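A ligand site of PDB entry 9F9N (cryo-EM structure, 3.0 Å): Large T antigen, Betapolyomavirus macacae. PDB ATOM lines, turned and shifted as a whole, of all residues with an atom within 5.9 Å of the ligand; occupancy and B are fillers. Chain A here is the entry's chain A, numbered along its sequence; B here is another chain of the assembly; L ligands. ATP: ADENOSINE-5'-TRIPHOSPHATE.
NZ of Lys 289 is in salt-bridge range of OD1 of Asp 286 (2.8 Å).
The guanidinium group of Arg 233 of chain B sits close to the side-chain amide nitrogen of Asn 264.
The side-chain amino group of Lys 167 lies within hydrogen-bond range of the side-chain amide oxygen of Asn 264.
The side-chain hydroxyl of Thr 168 lies within hydrogen-bond range of the side-chain carboxylate of Glu 208 (3.3 Å).
NZ of Lys 153 of chain B lies within salt-bridge range of OD2 of Asp 237 of chain B (2.9 Å).
The side-chain amino group (NZ) of Lys 285 lies within hydrogen-bond range of the backbone carbonyl oxygen (O) of Arg 283.
The backbone carbonyl oxygen of Leu 288 is in hydrogen-bond range of the indole nitrogen of Trp 128, at 3.3 Å.
N of Asn 264 lies within hydrogen-bond range of OD1 of Asp 209, 2.8 Å away.
The backbone carbonyl oxygen (O) of Pro 162 lies close to an oxygen (O1B) of the ligand (3.3 Å).
CD1 of Leu 132 touches N6 of the ligand, 3.5 Å away.
Ile 163 touches the ligand.
Glu 208 touches the ligand (OE2 to O2G, 3.8 Å).
O of Arg 283 touches N6 of the ligand, 3.9 Å away.
Pro 284 touches the ligand.
CD1 of Leu 288 touches N6 of the ligand, at 3.2 Å.
Lys 289 touches the ligand.
Leu 292 touches the ligand.
Hydrophobic or aromatic side chains within 4 Å of the ligand: Leu 132, Ile 163, Pro 284, Leu 288 and Leu 292.
20 residues have an atom within 4 Å of the ligand: Leu 132, Pro 162, Ile 163, Asp 164, Ser 165, Gly 166, Lys 167, Thr 168, Thr 169, Glu 208, Asn 264, Arg 283, Pro 284, Lys 285, Leu 288, Lys 289, Leu 292, Lys 153 of chain B, Arg 233 of chain B and Arg 275 of chain B.
The nearest printed residue that does not touch the ligand is Leu 299 (4.3 Å).
The backbone NH of Asp 164 sits at hydrogen-bond distance from an oxygen (O1B) of the ligand (3.2 Å).
An oxygen (O1B) of the ligand lies within salt-bridge range of the side-chain amino group (NZ) of Lys 167, at 2.5 Å.
O1A of the ligand is in hydrogen-bond range of N of Thr 169.
N of Ser 165 is in hydrogen-bond range of O1B of the ligand (3.0 Å).
NZ of Lys 153 of chain B lies within salt-bridge range of O2A of the ligand.
The side-chain hydroxyl of Thr 169 sits at hydrogen-bond distance from an oxygen (O1A) of the ligand.
N1 of the ligand sits at hydrogen-bond distance from N of Lys 285 (2.9 Å).
The backbone NH (N) of Lys 167 lies close to an oxygen (O2B) of the ligand (3.4 Å).
NH2 of Arg 275 of chain B lies within salt-bridge range of O1G of the ligand, at 2.8 Å.
OG1 of Thr 168 is in hydrogen-bond range of O2B of the ligand.
The backbone NH (N) of Thr 168 lies within hydrogen-bond range of an oxygen (O2B) of the ligand, 2.6 Å away.
N of Gly 166 sits close to N7 of the ligand (3.3 Å).
The guanidinium group (NH2) of Arg 233 of chain B is in salt-bridge range of an oxygen (O1G) of the ligand (2.6 Å).
An oxygen (O1B) of the ligand lies within hydrogen-bond range of the side-chain hydroxyl (OG) of Ser 165 (2.6 Å).
O3G of the ligand lies within hydrogen-bond range of ND2 of Asn 264 (2.8 Å).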
ATOM      1  N   TRP A 128     -23.639  24.418  25.246  1.00  0.00           N
ATOM      2  CA  TRP A 128     -23.777  22.990  24.935  1.00  0.00           C
ATOM      3  C   TRP A 128     -22.444  22.270  25.020  1.00  0.00           C
ATOM      4  O   TRP A 128     -22.320  21.223  25.667  1.00  0.00           O
ATOM      5  CB  TRP A 128     -24.377  22.794  23.547  1.00  0.00           C
ATOM      6  CG  TRP A 128     -24.700  21.331  23.225  1.00  0.00           C
ATOM      7  CD1 TRP A 128     -25.891  20.715  23.413  1.00  0.00           C
ATOM      8  CD2 TRP A 128     -23.813  20.333  22.675  1.00  0.00           C
ATOM      9  NE1 TRP A 128     -25.821  19.405  23.009  1.00  0.00           N
ATOM     10  CE2 TRP A 128     -24.562  19.146  22.549  1.00  0.00           C
ATOM     11  CE3 TRP A 128     -22.479  20.333  22.273  1.00  0.00           C
ATOM     12  CZ2 TRP A 128     -24.019  17.974  22.049  1.00  0.00           C
ATOM     13  CZ3 TRP A 128     -21.943  19.149  21.770  1.00  0.00           C
ATOM     14  CH2 TRP A 128     -22.715  17.994  21.667  1.00  0.00           C
ATOM     15  N   LEU A 132     -19.961  18.882  27.349  1.00  0.00           N
ATOM     16  CA  LEU A 132     -19.545  17.624  26.740  1.00  0.00           C
ATOM     17  C   LEU A 132     -18.673  16.796  27.680  1.00  0.00           C
ATOM     18  O   LEU A 132     -18.796  15.567  27.730  1.00  0.00           O
ATOM     19  CB  LEU A 132     -18.811  17.897  25.427  1.00  0.00           C
ATOM     20  CG  LEU A 132     -18.155  16.676  24.758  1.00  0.00           C
ATOM     21  CD1 LEU A 132     -19.186  15.616  24.398  1.00  0.00           C
ATOM     22  CD2 LEU A 132     -17.419  17.123  23.511  1.00  0.00           C
ATOM     23  N   PRO A 162     -17.841   5.174  22.978  1.00  0.00           N
ATOM     24  CA  PRO A 162     -18.602   4.555  21.891  1.00  0.00           C
ATOM     25  C   PRO A 162     -18.676   5.414  20.637  1.00  0.00           C
ATOM     26  O   PRO A 162     -17.954   6.404  20.497  1.00  0.00           O
ATOM     27  CB  PRO A 162     -19.992   4.379  22.526  1.00  0.00           C
ATOM     28  CG  PRO A 162     -20.111   5.544  23.431  1.00  0.00           C
ATOM     29  CD  PRO A 162     -18.713   5.817  23.967  1.00  0.00           C
ATOM     30  N   ILE A 163     -19.545   5.008  19.712  1.00  0.00           N
ATOM     31  CA  ILE A 163     -20.077   5.933  18.712  1.00  0.00           C
ATOM     32  C   ILE A 163     -20.924   7.020  19.383  1.00  0.00           C
ATOM     33  O   ILE A 163     -21.358   6.888  20.537  1.00  0.00           O
ATOM     34  CB  ILE A 163     -20.909   5.141  17.687  1.00  0.00           C
ATOM     35  CG1 ILE A 163     -21.372   6.036  16.534  1.00  0.00           C
ATOM     36  CG2 ILE A 163     -22.129   4.492  18.349  1.00  0.00           C
ATOM     37  CD1 ILE A 163     -21.761   5.247  15.282  1.00  0.00           C
ATOM     38  N   ASP A 164     -21.139   8.111  18.655  1.00  0.00           N
ATOM     39  CA  ASP A 164     -21.872   9.272  19.160  1.00  0.00           C
ATOM     40  C   ASP A 164     -21.299   9.789  20.472  1.00  0.00           C
ATOM     41  O   ASP A 164     -21.989  10.423  21.269  1.00  0.00           O
ATOM     42  CB  ASP A 164     -23.360   8.970  19.309  1.00  0.00           C
ATOM     43  CG  ASP A 164     -23.989   8.523  18.010  1.00  0.00           C
ATOM     44  OD1 ASP A 164     -23.417   8.832  16.940  1.00  0.00           O
ATOM     45  OD2 ASP A 164     -25.049   7.861  18.041  1.00  0.00           O
ATOM     46  N   SER A 165     -20.021   9.515  20.688  1.00  0.00           N
ATOM     47  CA  SER A 165     -19.304  10.010  21.849  1.00  0.00           C
ATOM     48  C   SER A 165     -18.906  11.469  21.713  1.00  0.00           C
ATOM     49  O   SER A 165     -18.451  12.068  22.690  1.00  0.00           O
ATOM     50  CB  SER A 165     -18.053   9.157  22.072  1.00  0.00           C
ATOM     51  OG  SER A 165     -17.137   9.357  21.002  1.00  0.00           O
ATOM     52  N   GLY A 166     -19.052  12.032  20.519  1.00  0.00           N
ATOM     53  CA  GLY A 166     -18.561  13.367  20.224  1.00  0.00           C
ATOM     54  C   GLY A 166     -17.078  13.436  19.951  1.00  0.00           C
ATOM     55  O   GLY A 166     -16.571  14.545  19.705  1.00  0.00           O
ATOM     56  N   LYS A 167     -16.364  12.314  19.981  1.00  0.00           N
ATOM     57  CA  LYS A 167     -14.907  12.394  19.907  1.00  0.00           C
ATOM     58  C   LYS A 167     -14.464  13.021  18.583  1.00  0.00           C
ATOM     59  O   LYS A 167     -13.520  13.807  18.549  1.00  0.00           O
ATOM     60  CB  LYS A 167     -14.299  11.012  20.113  1.00  0.00           C
ATOM     61  CG  LYS A 167     -14.665   9.980  19.079  1.00  0.00           C
ATOM     62  CD  LYS A 167     -14.230   8.589  19.493  1.00  0.00           C
ATOM     63  CE  LYS A 167     -14.718   7.553  18.482  1.00  0.00           C
ATOM     64  NZ  LYS A 167     -16.199   7.334  18.574  1.00  0.00           N
ATOM     65  N   THR A 168     -15.157  12.696  17.490  1.00  0.00           N
ATOM     66  CA  THR A 168     -14.887  13.396  16.235  1.00  0.00           C
ATOM     67  C   THR A 168     -15.338  14.852  16.302  1.00  0.00           C
ATOM     68  O   THR A 168     -14.687  15.732  15.729  1.00  0.00           O
ATOM     69  CB  THR A 168     -15.577  12.676  15.091  1.00  0.00           C
ATOM     70  OG1 THR A 168     -15.251  11.288  15.140  1.00  0.00           O
ATOM     71  CG2 THR A 168     -15.122  13.242  13.752  1.00  0.00           C
ATOM     72  N   THR A 169     -16.439  15.121  16.991  1.00  0.00           N
ATOM     73  CA  THR A 169     -16.875  16.508  17.185  1.00  0.00           C
ATOM     74  C   THR A 169     -15.787  17.327  17.855  1.00  0.00           C
ATOM     75  O   THR A 169     -15.533  18.474  17.476  1.00  0.00           O
ATOM     76  CB  THR A 169     -18.142  16.553  18.030  1.00  0.00           C
ATOM     77  OG1 THR A 169     -19.126  15.677  17.464  1.00  0.00           O
ATOM     78  CG2 THR A 169     -18.700  17.965  18.082  1.00  0.00           C
ATOM     79  N   LEU A 170     -15.149  16.760  18.871  1.00  0.00           N
ATOM     80  CA  LEU A 170     -14.057  17.461  19.545  1.00  0.00           C
ATOM     81  C   LEU A 170     -12.808  17.522  18.672  1.00  0.00           C
ATOM     82  O   LEU A 170     -12.158  18.565  18.587  1.00  0.00           O
ATOM     83  CB  LEU A 170     -13.749  16.770  20.869  1.00  0.00           C
ATOM     84  CG  LEU A 170     -12.673  17.434  21.709  1.00  0.00           C
ATOM     85  CD1 LEU A 170     -13.083  18.854  22.060  1.00  0.00           C
ATOM     86  CD2 LEU A 170     -12.456  16.628  22.966  1.00  0.00           C
ATOM     87  N   GLU A 208      -8.261   9.237  13.006  1.00  0.00           N
ATOM     88  CA  GLU A 208      -9.606   8.745  13.313  1.00  0.00           C
ATOM     89  C   GLU A 208      -9.637   7.243  13.618  1.00  0.00           C
ATOM     90  O   GLU A 208      -8.985   6.439  12.938  1.00  0.00           O
ATOM     91  CB  GLU A 208     -10.537   9.041  12.137  1.00  0.00           C
ATOM     92  CG  GLU A 208     -12.014   8.776  12.426  1.00  0.00           C
ATOM     93  CD  GLU A 208     -12.511   9.474  13.668  1.00  0.00           C
ATOM     94  OE1 GLU A 208     -12.316  10.699  13.792  1.00  0.00           O
ATOM     95  OE2 GLU A 208     -13.092   8.787  14.536  1.00  0.00           O
ATOM     96  N   ASP A 209     -10.397   6.892  14.643  1.00  0.00           N
ATOM     97  CA  ASP A 209     -10.691   5.511  15.057  1.00  0.00           C
ATOM     98  C   ASP A 209      -9.510   4.546  14.884  1.00  0.00           C
ATOM     99  O   ASP A 209      -9.534   3.607  14.093  1.00  0.00           O
ATOM    100  CB  ASP A 209     -11.927   4.972  14.353  1.00  0.00           C
ATOM    101  CG  ASP A 209     -12.627   3.886  15.155  1.00  0.00           C
ATOM    102  OD1 ASP A 209     -12.184   3.600  16.291  1.00  0.00           O
ATOM    103  OD2 ASP A 209     -13.625   3.315  14.665  1.00  0.00           O
ATOM    104  N   ASN A 264     -13.288   4.020  18.849  1.00  0.00           N
ATOM    105  CA  ASN A 264     -14.538   3.458  19.348  1.00  0.00           C
ATOM    106  C   ASN A 264     -14.267   2.347  20.354  1.00  0.00           C
ATOM    107  O   ASN A 264     -14.744   1.211  20.205  1.00  0.00           O
ATOM    108  CB  ASN A 264     -15.407   3.001  18.171  1.00  0.00           C
ATOM    109  CG  ASN A 264     -16.143   4.171  17.539  1.00  0.00           C
ATOM    110  OD1 ASN A 264     -16.988   4.794  18.181  1.00  0.00           O
ATOM    111  ND2 ASN A 264     -15.810   4.503  16.297  1.00  0.00           N
ATOM    112  N   ARG A 283     -18.924   9.492  26.751  1.00  0.00           N
ATOM    113  CA  ARG A 283     -20.144   8.667  26.654  1.00  0.00           C
ATOM    114  C   ARG A 283     -21.389   9.520  26.414  1.00  0.00           C
ATOM    115  O   ARG A 283     -21.533  10.583  27.031  1.00  0.00           O
ATOM    116  CB  ARG A 283     -20.321   7.814  27.915  1.00  0.00           C
ATOM    117  CG  ARG A 283     -19.112   6.932  28.190  1.00  0.00           C
ATOM    118  CD  ARG A 283     -19.273   6.059  29.426  1.00  0.00           C
ATOM    119  NE  ARG A 283     -17.970   5.552  29.854  1.00  0.00           N
ATOM    120  CZ  ARG A 283     -17.740   4.848  30.953  1.00  0.00           C
ATOM    121  NH1 ARG A 283     -18.725   4.467  31.748  1.00  0.00           N
ATOM    122  NH2 ARG A 283     -16.489   4.519  31.262  1.00  0.00           N
ATOM    123  N   PRO A 284     -22.312   9.072  25.555  1.00  0.00           N
ATOM    124  CA  PRO A 284     -23.519   9.865  25.272  1.00  0.00           C
ATOM    125  C   PRO A 284     -24.388  10.106  26.504  1.00  0.00           C
ATOM    126  O   PRO A 284     -24.426   9.294  27.424  1.00  0.00           O
ATOM    127  CB  PRO A 284     -24.262   9.029  24.229  1.00  0.00           C
ATOM    128  CG  PRO A 284     -23.255   8.113  23.644  1.00  0.00           C
ATOM    129  CD  PRO A 284     -22.209   7.889  24.692  1.00  0.00           C
ATOM    130  N   LYS A 285     -25.099  11.234  26.507  1.00  0.00           N
ATOM    131  CA  LYS A 285     -26.236  11.470  27.397  1.00  0.00           C
ATOM    132  C   LYS A 285     -27.430  12.026  26.629  1.00  0.00           C
ATOM    133  O   LYS A 285     -27.287  12.956  25.842  1.00  0.00           O
ATOM    134  CB  LYS A 285     -25.883  12.421  28.529  1.00  0.00           C
ATOM    135  CG  LYS A 285     -24.826  11.886  29.470  1.00  0.00           C
ATOM    136  CD  LYS A 285     -23.421  12.269  29.053  1.00  0.00           C
ATOM    137  CE  LYS A 285     -22.408  11.477  29.855  1.00  0.00           C
ATOM    138  NZ  LYS A 285     -20.996  11.762  29.457  1.00  0.00           N
ATOM    139  N   ASP A 286     -28.598  11.433  26.880  1.00  0.00           N
ATOM    140  CA  ASP A 286     -29.781  11.704  26.066  1.00  0.00           C
ATOM    141  C   ASP A 286     -30.210  13.169  26.117  1.00  0.00           C
ATOM    142  O   ASP A 286     -30.680  13.713  25.113  1.00  0.00           O
ATOM    143  CB  ASP A 286     -30.941  10.819  26.529  1.00  0.00           C
ATOM    144  CG  ASP A 286     -30.681   9.357  26.301  1.00  0.00           C
ATOM    145  OD1 ASP A 286     -29.814   9.029  25.465  1.00  0.00           O
ATOM    146  OD2 ASP A 286     -31.334   8.524  26.967  1.00  0.00           O
ATOM    147  N   LEU A 288     -28.404  15.742  26.154  1.00  0.00           N
ATOM    148  CA  LEU A 288     -27.632  16.469  25.154  1.00  0.00           C
ATOM    149  C   LEU A 288     -28.225  16.260  23.768  1.00  0.00           C
ATOM    150  O   LEU A 288     -28.349  17.213  22.990  1.00  0.00           O
ATOM    151  CB  LEU A 288     -26.180  16.018  25.214  1.00  0.00           C
ATOM    152  CG  LEU A 288     -25.534  16.189  26.599  1.00  0.00           C
ATOM    153  CD1 LEU A 288     -24.130  15.605  26.639  1.00  0.00           C
ATOM    154  CD2 LEU A 288     -25.497  17.666  26.985  1.00  0.00           C
ATOM    155  N   LYS A 289     -28.626  15.034  23.466  1.00  0.00           N
ATOM    156  CA  LYS A 289     -29.318  14.770  22.203  1.00  0.00           C
ATOM    157  C   LYS A 289     -30.593  15.588  22.087  1.00  0.00           C
ATOM    158  O   LYS A 289     -30.811  16.302  21.103  1.00  0.00           O
ATOM    159  CB  LYS A 289     -29.652  13.289  22.097  1.00  0.00           C
ATOM    160  CG  LYS A 289     -28.519  12.356  22.454  1.00  0.00           C
ATOM    161  CD  LYS A 289     -28.969  10.912  22.363  1.00  0.00           C
ATOM    162  CE  LYS A 289     -27.886   9.956  22.836  1.00  0.00           C
ATOM    163  NZ  LYS A 289     -28.418   8.585  23.097  1.00  0.00           N
ATOM    164  N   LEU A 292     -29.833  19.183  21.345  1.00  0.00           N
ATOM    165  CA  LEU A 292     -29.594  19.361  19.919  1.00  0.00           C
ATOM    166  C   LEU A 292     -30.895  19.326  19.147  1.00  0.00           C
ATOM    167  O   LEU A 292     -31.176  20.204  18.323  1.00  0.00           O
ATOM    168  CB  LEU A 292     -28.680  18.252  19.395  1.00  0.00           C
ATOM    169  CG  LEU A 292     -27.258  18.182  19.931  1.00  0.00           C
ATOM    170  CD1 LEU A 292     -26.610  16.890  19.491  1.00  0.00           C
ATOM    171  CD2 LEU A 292     -26.452  19.380  19.464  1.00  0.00           C
ATOM    172  N   LEU A 299     -26.476  22.291  15.108  1.00  0.00           N
ATOM    173  CA  LEU A 299     -25.935  21.432  14.068  1.00  0.00           C
ATOM    174  C   LEU A 299     -26.046  22.057  12.698  1.00  0.00           C
ATOM    175  O   LEU A 299     -25.089  21.996  11.919  1.00  0.00           O
ATOM    176  CB  LEU A 299     -26.626  20.069  14.106  1.00  0.00           C
ATOM    177  CG  LEU A 299     -26.048  19.121  15.165  1.00  0.00           C
ATOM    178  CD1 LEU A 299     -26.960  17.939  15.385  1.00  0.00           C
ATOM    179  CD2 LEU A 299     -24.673  18.631  14.748  1.00  0.00           C
ATOM    180  N   ILE A 304     -21.408  23.464  16.832  1.00  0.00           N
ATOM    181  CA  ILE A 304     -20.762  22.556  17.768  1.00  0.00           C
ATOM    182  C   ILE A 304     -19.620  21.754  17.149  1.00  0.00           C
ATOM    183  O   ILE A 304     -18.913  21.055  17.886  1.00  0.00           O
ATOM    184  CB  ILE A 304     -21.792  21.620  18.431  1.00  0.00           C
ATOM    185  CG1 ILE A 304     -22.425  20.663  17.431  1.00  0.00           C
ATOM    186  CG2 ILE A 304     -22.849  22.427  19.148  1.00  0.00           C
ATOM    187  CD1 ILE A 304     -22.819  19.347  18.062  1.00  0.00           C
ATOM    188  N   LYS B 153     -23.958  14.004   9.189  1.00  0.00           N
ATOM    189  CA  LYS B 153     -24.521  12.700   9.563  1.00  0.00           C
ATOM    190  C   LYS B 153     -26.016  12.598   9.242  1.00  0.00           C
ATOM    191  O   LYS B 153     -26.717  11.764   9.810  1.00  0.00           O
ATOM    192  CB  LYS B 153     -24.260  12.366  11.031  1.00  0.00           C
ATOM    193  CG  LYS B 153     -22.795  12.552  11.418  1.00  0.00           C
ATOM    194  CD  LYS B 153     -22.330  11.561  12.477  1.00  0.00           C
ATOM    195  CE  LYS B 153     -20.891  11.861  12.900  1.00  0.00           C
ATOM    196  NZ  LYS B 153     -20.194  10.677  13.474  1.00  0.00           N
ATOM    197  N   ARG B 233     -17.151   5.915   6.709  1.00  0.00           N
ATOM    198  CA  ARG B 233     -18.129   6.579   7.574  1.00  0.00           C
ATOM    199  C   ARG B 233     -17.992   8.096   7.603  1.00  0.00           C
ATOM    200  O   ARG B 233     -18.992   8.819   7.596  1.00  0.00           O
ATOM    201  CB  ARG B 233     -17.970   6.026   8.982  1.00  0.00           C
ATOM    202  CG  ARG B 233     -18.549   4.630   9.146  1.00  0.00           C
ATOM    203  CD  ARG B 233     -17.940   3.916  10.338  1.00  0.00           C
ATOM    204  NE  ARG B 233     -18.068   4.635  11.604  1.00  0.00           N
ATOM    205  CZ  ARG B 233     -18.012   4.057  12.796  1.00  0.00           C
ATOM    206  NH1 ARG B 233     -17.872   2.753  12.927  1.00  0.00           N
ATOM    207  NH2 ARG B 233     -18.152   4.813  13.886  1.00  0.00           N
ATOM    208  N   ASP B 237     -20.663  10.849   6.991  1.00  0.00           N
ATOM    209  CA  ASP B 237     -20.967  11.817   8.027  1.00  0.00           C
ATOM    210  C   ASP B 237     -20.828  13.238   7.521  1.00  0.00           C
ATOM    211  O   ASP B 237     -21.506  14.145   8.027  1.00  0.00           O
ATOM    212  CB  ASP B 237     -20.055  11.595   9.217  1.00  0.00           C
ATOM    213  CG  ASP B 237     -20.370  10.308   9.964  1.00  0.00           C
ATOM    214  OD1 ASP B 237     -21.439   9.723   9.711  1.00  0.00           O
ATOM    215  OD2 ASP B 237     -19.535   9.879  10.796  1.00  0.00           O
ATOM    216  N   SER B 239     -18.441  15.054   8.247  1.00  0.00           N
ATOM    217  CA  SER B 239     -18.057  15.738   9.464  1.00  0.00           C
ATOM    218  C   SER B 239     -16.951  16.749   9.199  1.00  0.00           C
ATOM    219  O   SER B 239     -16.946  17.836   9.779  1.00  0.00           O
ATOM    220  CB  SER B 239     -17.612  14.735  10.516  1.00  0.00           C
ATOM    221  OG  SER B 239     -17.311  15.391  11.733  1.00  0.00           O
ATOM    222  N   ARG B 275     -26.529   5.672   9.848  1.00  0.00           N
ATOM    223  CA  ARG B 275     -26.031   6.835   9.128  1.00  0.00           C
ATOM    224  C   ARG B 275     -26.952   7.377   8.040  1.00  0.00           C
ATOM    225  O   ARG B 275     -26.886   8.565   7.729  1.00  0.00           O
ATOM    226  CB  ARG B 275     -24.650   6.524   8.557  1.00  0.00           C
ATOM    227  CG  ARG B 275     -23.583   6.684   9.609  1.00  0.00           C
ATOM    228  CD  ARG B 275     -22.196   6.400   9.085  1.00  0.00           C
ATOM    229  NE  ARG B 275     -21.184   7.049   9.895  1.00  0.00           N
ATOM    230  CZ  ARG B 275     -20.798   6.663  11.100  1.00  0.00           C
ATOM    231  NH1 ARG B 275     -21.240   5.534  11.645  1.00  0.00           N
ATOM    232  NH2 ARG B 275     -19.893   7.382  11.751  1.00  0.00           N
HETATM  233  PG  ATP L   1     -17.676   8.026  15.035  1.00  0.00           P
HETATM  234  O1G ATP L   1     -18.728   7.307  14.270  1.00  0.00           O
HETATM  235  O2G ATP L   1     -16.897   8.955  14.110  1.00  0.00           O
HETATM  236  O3G ATP L   1     -16.848   7.079  15.883  1.00  0.00           O
HETATM  237  PB  ATP L   1     -17.963   9.844  17.313  1.00  0.00           P
HETATM  238  O1B ATP L   1     -18.027   9.037  18.536  1.00  0.00           O
HETATM  239  O2B ATP L   1     -16.611  10.525  17.099  1.00  0.00           O
HETATM  240  O3B ATP L   1     -18.352   8.993  16.078  1.00  0.00           O
HETATM  241  PA  ATP L   1     -19.206  12.402  16.714  1.00  0.00           P
HETATM  242  O1A ATP L   1     -18.321  13.383  17.352  1.00  0.00           O
HETATM  243  O2A ATP L   1     -19.017  12.313  15.209  1.00  0.00           O
HETATM  244  O3A ATP L   1     -19.059  10.988  17.324  1.00  0.00           O
HETATM  245  O5' ATP L   1     -20.701  12.805  17.043  1.00  0.00           O
HETATM  246  C5' ATP L   1     -21.802  12.279  16.277  1.00  0.00           C
HETATM  247  C4' ATP L   1     -23.071  12.547  17.016  1.00  0.00           C
HETATM  248  O4' ATP L   1     -22.956  12.050  18.360  1.00  0.00           O
HETATM  249  C3' ATP L   1     -23.287  14.026  17.248  1.00  0.00           C
HETATM  250  O3' ATP L   1     -23.848  14.660  16.103  1.00  0.00           O
HETATM  251  C2' ATP L   1     -24.265  14.036  18.418  1.00  0.00           C
HETATM  252  O2' ATP L   1     -25.597  13.937  17.935  1.00  0.00           O
HETATM  253  C1' ATP L   1     -23.887  12.747  19.182  1.00  0.00           C
HETATM  254  N9  ATP L   1     -23.200  13.068  20.420  1.00  0.00           N
HETATM  255  C8  ATP L   1     -21.937  13.577  20.569  1.00  0.00           C
HETATM  256  N7  ATP L   1     -21.594  13.783  21.815  1.00  0.00           N
HETATM  257  C5  ATP L   1     -22.716  13.398  22.530  1.00  0.00           C
HETATM  258  C6  ATP L   1     -22.996  13.368  23.908  1.00  0.00           C
HETATM  259  N6  ATP L   1     -22.135  13.765  24.855  1.00  0.00           N
HETATM  260  N1  ATP L   1     -24.206  12.922  24.302  1.00  0.00           N
HETATM  261  C2  ATP L   1     -25.077  12.521  23.364  1.00  0.00           C
HETATM  262  N3  ATP L   1     -24.920  12.501  22.033  1.00  0.00           N
HETATM  263  C4  ATP L   1     -23.706  12.941  21.689  1.00  0.00           C
